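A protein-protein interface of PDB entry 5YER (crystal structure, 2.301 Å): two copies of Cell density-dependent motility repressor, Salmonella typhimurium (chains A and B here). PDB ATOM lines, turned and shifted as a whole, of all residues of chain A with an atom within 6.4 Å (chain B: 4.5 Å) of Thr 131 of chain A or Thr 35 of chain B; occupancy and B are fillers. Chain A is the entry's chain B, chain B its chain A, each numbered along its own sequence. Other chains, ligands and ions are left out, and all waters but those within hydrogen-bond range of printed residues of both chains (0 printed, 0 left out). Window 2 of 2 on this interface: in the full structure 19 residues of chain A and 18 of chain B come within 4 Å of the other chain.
Thr 131 of chain A touches Thr 35 of chain B (O to CG2, 3.4 Å).
CE1 of Phe 132 of chain A touches O of Phe 34 of chain B, at 3.5 Å.
O of Phe 132 of chain A touches CA of Thr 35 of chain B, 3.7 Å away.
Phe 133 of chain A touches Tyr 36 of chain B (CA to O, 3.4 Å).
Ala 37 of chain B touches Val 134 of chain A.
Phe 102 of chain A touches none of the printed residues of chain B.
Of the printed residues of chain B, Val 134 of chain A touches Tyr 36 (2.9 Å) and Ala 37 (3.7 Å).
Of the printed residues of chain A, Phe 34 of chain B touches Phe 132.
Of the printed residues of chain A, Thr 35 of chain B touches Thr 131 (3.4 Å) and Phe 132 (3.7 Å).
No position is printed for both chains.
The backbone carbonyl oxygen of Arg 8 of chain B sits at hydrogen-bond distance from the backbone NH of Thr 35 of chain B.
The backbone NH of Ile 10 of chain B is in hydrogen-bond range of the backbone carbonyl oxygen of Thr 35 of chain B (2.4 Å).
The backbone carbonyl oxygen of Ile 10 of chain B lies within hydrogen-bond range of the backbone NH of Ala 37 of chain B (3.1 Å).
N of Phe 132 of chain A is in hydrogen-bond range of O of Leu 104 of chain A, 3.0 Å away.
The backbone carbonyl oxygen (O) of Leu 104 of chain A sits at hydrogen-bond distance from the backbone NH (N) of Phe 133 of chain A (3.4 Å).
O of Phe 133 of chain A sits at hydrogen-bond distance from N of Asn 106 of chain A, 3.0 Å away.
The backbone NH (N) of Tyr 36 of chain B lies within hydrogen-bond range of the backbone carbonyl oxygen (O) of Phe 132 of chain A (2.9 Å).
N of Val 134 of chain A is in hydrogen-bond range of O of Tyr 36 of chain B.
Of the 7 printed residues of chain B, 4 touch a printed residue of chain A.
Printed residues of chain B that touch a printed residue of chain A: Phe 34, Thr 35, Tyr 36 and Ala 37.
Hydrophobic or aromatic side chains of chain B that line the printed part of chain A: Tyr 36.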
ATOM      1  N   HIS A 101      -7.880 -22.828 -12.062  1.00  0.00           N
ATOM      2  CA  HIS A 101      -8.219 -22.695 -10.645  1.00  0.00           C
ATOM      3  C   HIS A 101      -9.428 -21.771 -10.459  1.00  0.00           C
ATOM      4  O   HIS A 101      -9.346 -20.685  -9.880  1.00  0.00           O
ATOM      5  CB  HIS A 101      -7.008 -22.211  -9.837  1.00  0.00           C
ATOM      6  CG  HIS A 101      -6.022 -23.293  -9.523  1.00  0.00           C
ATOM      7  ND1 HIS A 101      -6.175 -24.156  -8.459  1.00  0.00           N
ATOM      8  CD2 HIS A 101      -4.870 -23.656 -10.137  1.00  0.00           C
ATOM      9  CE1 HIS A 101      -5.159 -25.000  -8.429  1.00  0.00           C
ATOM     10  NE2 HIS A 101      -4.353 -24.718  -9.437  1.00  0.00           N
ATOM     11  N   PHE A 102     -10.570 -22.243 -10.976  1.00  0.00           N
ATOM     12  CA  PHE A 102     -11.800 -21.484 -10.822  1.00  0.00           C
ATOM     13  C   PHE A 102     -12.332 -21.617  -9.396  1.00  0.00           C
ATOM     14  O   PHE A 102     -12.073 -22.616  -8.720  1.00  0.00           O
ATOM     15  CB  PHE A 102     -12.858 -21.950 -11.826  1.00  0.00           C
ATOM     16  CG  PHE A 102     -13.336 -23.367 -11.616  1.00  0.00           C
ATOM     17  CD1 PHE A 102     -14.363 -23.650 -10.727  1.00  0.00           C
ATOM     18  CD2 PHE A 102     -12.774 -24.410 -12.330  1.00  0.00           C
ATOM     19  CE1 PHE A 102     -14.803 -24.949 -10.543  1.00  0.00           C
ATOM     20  CE2 PHE A 102     -13.210 -25.710 -12.151  1.00  0.00           C
ATOM     21  CZ  PHE A 102     -14.226 -25.979 -11.257  1.00  0.00           C
ATOM     22  N   PRO A 103     -13.071 -20.617  -8.914  1.00  0.00           N
ATOM     23  CA  PRO A 103     -13.638 -20.705  -7.560  1.00  0.00           C
ATOM     24  C   PRO A 103     -14.664 -21.826  -7.471  1.00  0.00           C
ATOM     25  O   PRO A 103     -15.605 -21.891  -8.265  1.00  0.00           O
ATOM     26  CB  PRO A 103     -14.287 -19.330  -7.354  1.00  0.00           C
ATOM     27  CG  PRO A 103     -13.641 -18.438  -8.367  1.00  0.00           C
ATOM     28  CD  PRO A 103     -13.345 -19.313  -9.542  1.00  0.00           C
ATOM     29  N   LEU A 104     -14.474 -22.709  -6.496  1.00  0.00           N
ATOM     30  CA  LEU A 104     -15.340 -23.863  -6.298  1.00  0.00           C
ATOM     31  C   LEU A 104     -16.120 -23.709  -5.001  1.00  0.00           C
ATOM     32  O   LEU A 104     -15.538 -23.422  -3.950  1.00  0.00           O
ATOM     33  CB  LEU A 104     -14.531 -25.162  -6.267  1.00  0.00           C
ATOM     34  CG  LEU A 104     -15.328 -26.408  -5.871  1.00  0.00           C
ATOM     35  CD1 LEU A 104     -16.395 -26.716  -6.910  1.00  0.00           C
ATOM     36  CD2 LEU A 104     -14.416 -27.606  -5.661  1.00  0.00           C
ATOM     37  N   LEU A 105     -17.432 -23.905  -5.081  1.00  0.00           N
ATOM     38  CA  LEU A 105     -18.310 -23.961  -3.914  1.00  0.00           C
ATOM     39  C   LEU A 105     -18.752 -25.415  -3.777  1.00  0.00           C
ATOM     40  O   LEU A 105     -19.610 -25.886  -4.529  1.00  0.00           O
ATOM     41  CB  LEU A 105     -19.493 -23.016  -4.073  1.00  0.00           C
ATOM     42  CG  LEU A 105     -19.179 -21.684  -4.757  1.00  0.00           C
ATOM     43  CD1 LEU A 105     -20.450 -20.892  -4.985  1.00  0.00           C
ATOM     44  CD2 LEU A 105     -18.185 -20.875  -3.938  1.00  0.00           C
ATOM     45  N   ASN A 106     -18.162 -26.124  -2.822  1.00  0.00           N
ATOM     46  CA  ASN A 106     -18.315 -27.567  -2.722  1.00  0.00           C
ATOM     47  C   ASN A 106     -18.926 -27.955  -1.383  1.00  0.00           C
ATOM     48  O   ASN A 106     -18.932 -27.178  -0.423  1.00  0.00           O
ATOM     49  CB  ASN A 106     -16.962 -28.272  -2.900  1.00  0.00           C
ATOM     50  CG  ASN A 106     -17.111 -29.732  -3.276  1.00  0.00           C
ATOM     51  OD1 ASN A 106     -18.184 -30.170  -3.692  1.00  0.00           O
ATOM     52  ND2 ASN A 106     -16.034 -30.494  -3.130  1.00  0.00           N
ATOM     53  N   GLN A 109     -16.178 -32.607   3.014  1.00  0.00           N
ATOM     54  CA  GLN A 109     -15.551 -33.888   2.706  1.00  0.00           C
ATOM     55  C   GLN A 109     -16.336 -35.055   3.289  1.00  0.00           C
ATOM     56  O   GLN A 109     -16.321 -36.156   2.728  1.00  0.00           O
ATOM     57  CB  GLN A 109     -14.115 -33.911   3.231  1.00  0.00           C
ATOM     58  CG  GLN A 109     -13.318 -32.653   2.933  1.00  0.00           C
ATOM     59  CD  GLN A 109     -12.821 -32.605   1.503  1.00  0.00           C
ATOM     60  OE1 GLN A 109     -12.094 -33.493   1.056  1.00  0.00           O
ATOM     61  NE2 GLN A 109     -13.209 -31.564   0.775  1.00  0.00           N
ATOM     62  N   PHE A 129      -9.365 -26.176 -10.209  1.00  0.00           N
ATOM     63  CA  PHE A 129     -10.273 -25.419  -9.361  1.00  0.00           C
ATOM     64  C   PHE A 129      -9.551 -24.967  -8.098  1.00  0.00           C
ATOM     65  O   PHE A 129      -8.458 -25.434  -7.773  1.00  0.00           O
ATOM     66  CB  PHE A 129     -11.515 -26.245  -8.996  1.00  0.00           C
ATOM     67  CG  PHE A 129     -11.205 -27.524  -8.270  1.00  0.00           C
ATOM     68  CD1 PHE A 129     -11.146 -27.556  -6.885  1.00  0.00           C
ATOM     69  CD2 PHE A 129     -10.973 -28.695  -8.972  1.00  0.00           C
ATOM     70  CE1 PHE A 129     -10.861 -28.732  -6.215  1.00  0.00           C
ATOM     71  CE2 PHE A 129     -10.687 -29.874  -8.307  1.00  0.00           C
ATOM     72  CZ  PHE A 129     -10.631 -29.891  -6.927  1.00  0.00           C
ATOM     73  N   SER A 130     -10.190 -24.042  -7.384  1.00  0.00           N
ATOM     74  CA  SER A 130      -9.703 -23.548  -6.102  1.00  0.00           C
ATOM     75  C   SER A 130     -10.874 -23.508  -5.133  1.00  0.00           C
ATOM     76  O   SER A 130     -11.834 -22.759  -5.347  1.00  0.00           O
ATOM     77  CB  SER A 130      -9.069 -22.162  -6.243  1.00  0.00           C
ATOM     78  OG  SER A 130      -8.509 -21.731  -5.015  1.00  0.00           O
ATOM     79  N   THR A 131     -10.798 -24.313  -4.076  1.00  0.00           N
ATOM     80  CA  THR A 131     -11.891 -24.424  -3.115  1.00  0.00           C
ATOM     81  C   THR A 131     -12.020 -23.122  -2.331  1.00  0.00           C
ATOM     82  O   THR A 131     -11.125 -22.758  -1.563  1.00  0.00           O
ATOM     83  CB  THR A 131     -11.651 -25.604  -2.180  1.00  0.00           C
ATOM     84  OG1 THR A 131     -11.631 -26.819  -2.940  1.00  0.00           O
ATOM     85  CG2 THR A 131     -12.751 -25.686  -1.146  1.00  0.00           C
ATOM     86  N   PHE A 132     -13.139 -22.423  -2.520  1.00  0.00           N
ATOM     87  CA  PHE A 132     -13.376 -21.129  -1.894  1.00  0.00           C
ATOM     88  C   PHE A 132     -14.399 -21.168  -0.769  1.00  0.00           C
ATOM     89  O   PHE A 132     -14.251 -20.430   0.207  1.00  0.00           O
ATOM     90  CB  PHE A 132     -13.832 -20.110  -2.949  1.00  0.00           C
ATOM     91  CG  PHE A 132     -14.424 -18.855  -2.372  1.00  0.00           C
ATOM     92  CD1 PHE A 132     -13.619 -17.909  -1.761  1.00  0.00           C
ATOM     93  CD2 PHE A 132     -15.787 -18.619  -2.448  1.00  0.00           C
ATOM     94  CE1 PHE A 132     -14.162 -16.753  -1.231  1.00  0.00           C
ATOM     95  CE2 PHE A 132     -16.336 -17.466  -1.920  1.00  0.00           C
ATOM     96  CZ  PHE A 132     -15.522 -16.532  -1.311  1.00  0.00           C
ATOM     97  N   PHE A 133     -15.424 -22.012  -0.875  1.00  0.00           N
ATOM     98  CA  PHE A 133     -16.486 -22.083   0.120  1.00  0.00           C
ATOM     99  C   PHE A 133     -16.903 -23.534   0.298  1.00  0.00           C
ATOM    100  O   PHE A 133     -17.159 -24.232  -0.688  1.00  0.00           O
ATOM    101  CB  PHE A 133     -17.688 -21.227  -0.303  1.00  0.00           C
ATOM    102  CG  PHE A 133     -18.718 -21.045   0.774  1.00  0.00           C
ATOM    103  CD1 PHE A 133     -19.735 -21.970   0.944  1.00  0.00           C
ATOM    104  CD2 PHE A 133     -18.674 -19.944   1.613  1.00  0.00           C
ATOM    105  CE1 PHE A 133     -20.684 -21.805   1.933  1.00  0.00           C
ATOM    106  CE2 PHE A 133     -19.621 -19.772   2.604  1.00  0.00           C
ATOM    107  CZ  PHE A 133     -20.627 -20.704   2.763  1.00  0.00           C
ATOM    108  N   VAL A 134     -16.975 -23.985   1.550  1.00  0.00           N
ATOM    109  CA  VAL A 134     -17.317 -25.365   1.874  1.00  0.00           C
ATOM    110  C   VAL A 134     -18.477 -25.372   2.859  1.00  0.00           C
ATOM    111  O   VAL A 134     -18.414 -24.717   3.905  1.00  0.00           O
ATOM    112  CB  VAL A 134     -16.114 -26.133   2.457  1.00  0.00           C
ATOM    113  CG1 VAL A 134     -16.579 -27.413   3.136  1.00  0.00           C
ATOM    114  CG2 VAL A 134     -15.119 -26.454   1.365  1.00  0.00           C
ATOM    115  N   ARG B   8      -5.116 -19.134   4.604  1.00  0.00           N
ATOM    116  CA  ARG B   8      -6.267 -18.318   4.258  1.00  0.00           C
ATOM    117  C   ARG B   8      -7.600 -18.914   4.679  1.00  0.00           C
ATOM    118  O   ARG B   8      -8.595 -18.184   4.704  1.00  0.00           O
ATOM    119  CB  ARG B   8      -6.295 -18.054   2.746  1.00  0.00           C
ATOM    120  CG  ARG B   8      -4.979 -17.588   2.145  1.00  0.00           C
ATOM    121  CD  ARG B   8      -5.164 -17.108   0.713  1.00  0.00           C
ATOM    122  NE  ARG B   8      -5.234 -15.651   0.619  1.00  0.00           N
ATOM    123  CZ  ARG B   8      -4.870 -14.953  -0.453  1.00  0.00           C
ATOM    124  NH1 ARG B   8      -4.414 -15.580  -1.528  1.00  0.00           N
ATOM    125  NH2 ARG B   8      -4.961 -13.629  -0.452  1.00  0.00           N
ATOM    126  N   LYS B   9      -7.655 -20.202   5.016  1.00  0.00           N
ATOM    127  CA  LYS B   9      -8.937 -20.829   5.310  1.00  0.00           C
ATOM    128  C   LYS B   9      -9.468 -20.369   6.661  1.00  0.00           C
ATOM    129  O   LYS B   9      -8.761 -20.425   7.672  1.00  0.00           O
ATOM    130  CB  LYS B   9      -8.817 -22.351   5.291  1.00  0.00           C
ATOM    131  CG  LYS B   9     -10.134 -23.062   5.551  1.00  0.00           C
ATOM    132  CD  LYS B   9      -9.927 -24.524   5.901  1.00  0.00           C
ATOM    133  CE  LYS B   9      -9.245 -25.262   4.767  1.00  0.00           C
ATOM    134  NZ  LYS B   9      -9.109 -26.719   5.048  1.00  0.00           N
ATOM    135  N   ILE B  10     -10.719 -19.917   6.672  1.00  0.00           N
ATOM    136  CA  ILE B  10     -11.413 -19.492   7.882  1.00  0.00           C
ATOM    137  C   ILE B  10     -12.440 -20.565   8.217  1.00  0.00           C
ATOM    138  O   ILE B  10     -13.410 -20.764   7.474  1.00  0.00           O
ATOM    139  CB  ILE B  10     -12.079 -18.121   7.706  1.00  0.00           C
ATOM    140  CG1 ILE B  10     -11.045 -17.067   7.299  1.00  0.00           C
ATOM    141  CG2 ILE B  10     -12.799 -17.709   8.981  1.00  0.00           C
ATOM    142  CD1 ILE B  10      -9.925 -16.891   8.299  1.00  0.00           C
ATOM    143  N   PHE B  34      -9.971 -14.632   1.797  1.00  0.00           N
ATOM    144  CA  PHE B  34     -10.275 -15.718   2.716  1.00  0.00           C
ATOM    145  C   PHE B  34     -10.812 -16.925   1.961  1.00  0.00           C
ATOM    146  O   PHE B  34     -11.311 -16.817   0.839  1.00  0.00           O
ATOM    147  CB  PHE B  34     -11.293 -15.287   3.783  1.00  0.00           C
ATOM    148  CG  PHE B  34     -10.923 -14.021   4.499  1.00  0.00           C
ATOM    149  CD1 PHE B  34      -9.847 -13.993   5.368  1.00  0.00           C
ATOM    150  CD2 PHE B  34     -11.652 -12.859   4.304  1.00  0.00           C
ATOM    151  CE1 PHE B  34      -9.500 -12.831   6.027  1.00  0.00           C
ATOM    152  CE2 PHE B  34     -11.310 -11.693   4.960  1.00  0.00           C
ATOM    153  CZ  PHE B  34     -10.232 -11.679   5.822  1.00  0.00           C
ATOM    154  N   THR B  35     -10.702 -18.080   2.613  1.00  0.00           N
ATOM    155  CA  THR B  35     -11.346 -19.318   2.201  1.00  0.00           C
ATOM    156  C   THR B  35     -12.243 -19.783   3.341  1.00  0.00           C
ATOM    157  O   THR B  35     -11.832 -19.774   4.505  1.00  0.00           O
ATOM    158  CB  THR B  35     -10.312 -20.400   1.854  1.00  0.00           C
ATOM    159  OG1 THR B  35      -9.634 -20.044   0.643  1.00  0.00           O
ATOM    160  CG2 THR B  35     -10.984 -21.757   1.664  1.00  0.00           C
ATOM    161  N   TYR B  36     -13.469 -20.179   3.011  1.00  0.00           N
ATOM    162  CA  TYR B  36     -14.498 -20.440   4.010  1.00  0.00           C
ATOM    163  C   TYR B  36     -14.784 -21.932   4.115  1.00  0.00           C
ATOM    164  O   TYR B  36     -14.933 -22.615   3.096  1.00  0.00           O
ATOM    165  CB  TYR B  36     -15.783 -19.684   3.675  1.00  0.00           C
ATOM    166  CG  TYR B  36     -15.609 -18.185   3.603  1.00  0.00           C
ATOM    167  CD1 TYR B  36     -15.754 -17.397   4.735  1.00  0.00           C
ATOM    168  CD2 TYR B  36     -15.299 -17.559   2.403  1.00  0.00           C
ATOM    169  CE1 TYR B  36     -15.596 -16.024   4.677  1.00  0.00           C
ATOM    170  CE2 TYR B  36     -15.139 -16.187   2.333  1.00  0.00           C
ATOM    171  CZ  TYR B  36     -15.289 -15.426   3.474  1.00  0.00           C
ATOM    172  OH  TYR B  36     -15.132 -14.060   3.410  1.00  0.00           O
ATOM    173  N   ALA B  37     -14.863 -22.425   5.349  1.00  0.00           N
ATOM    174  CA  ALA B  37     -15.295 -23.787   5.647  1.00  0.00           C
ATOM    175  C   ALA B  37     -16.342 -23.696   6.749  1.00  0.00           C
ATOM    176  O   ALA B  37     -16.001 -23.461   7.914  1.00  0.00           O
ATOM    177  CB  ALA B  37     -14.121 -24.670   6.071  1.00  0.00           C
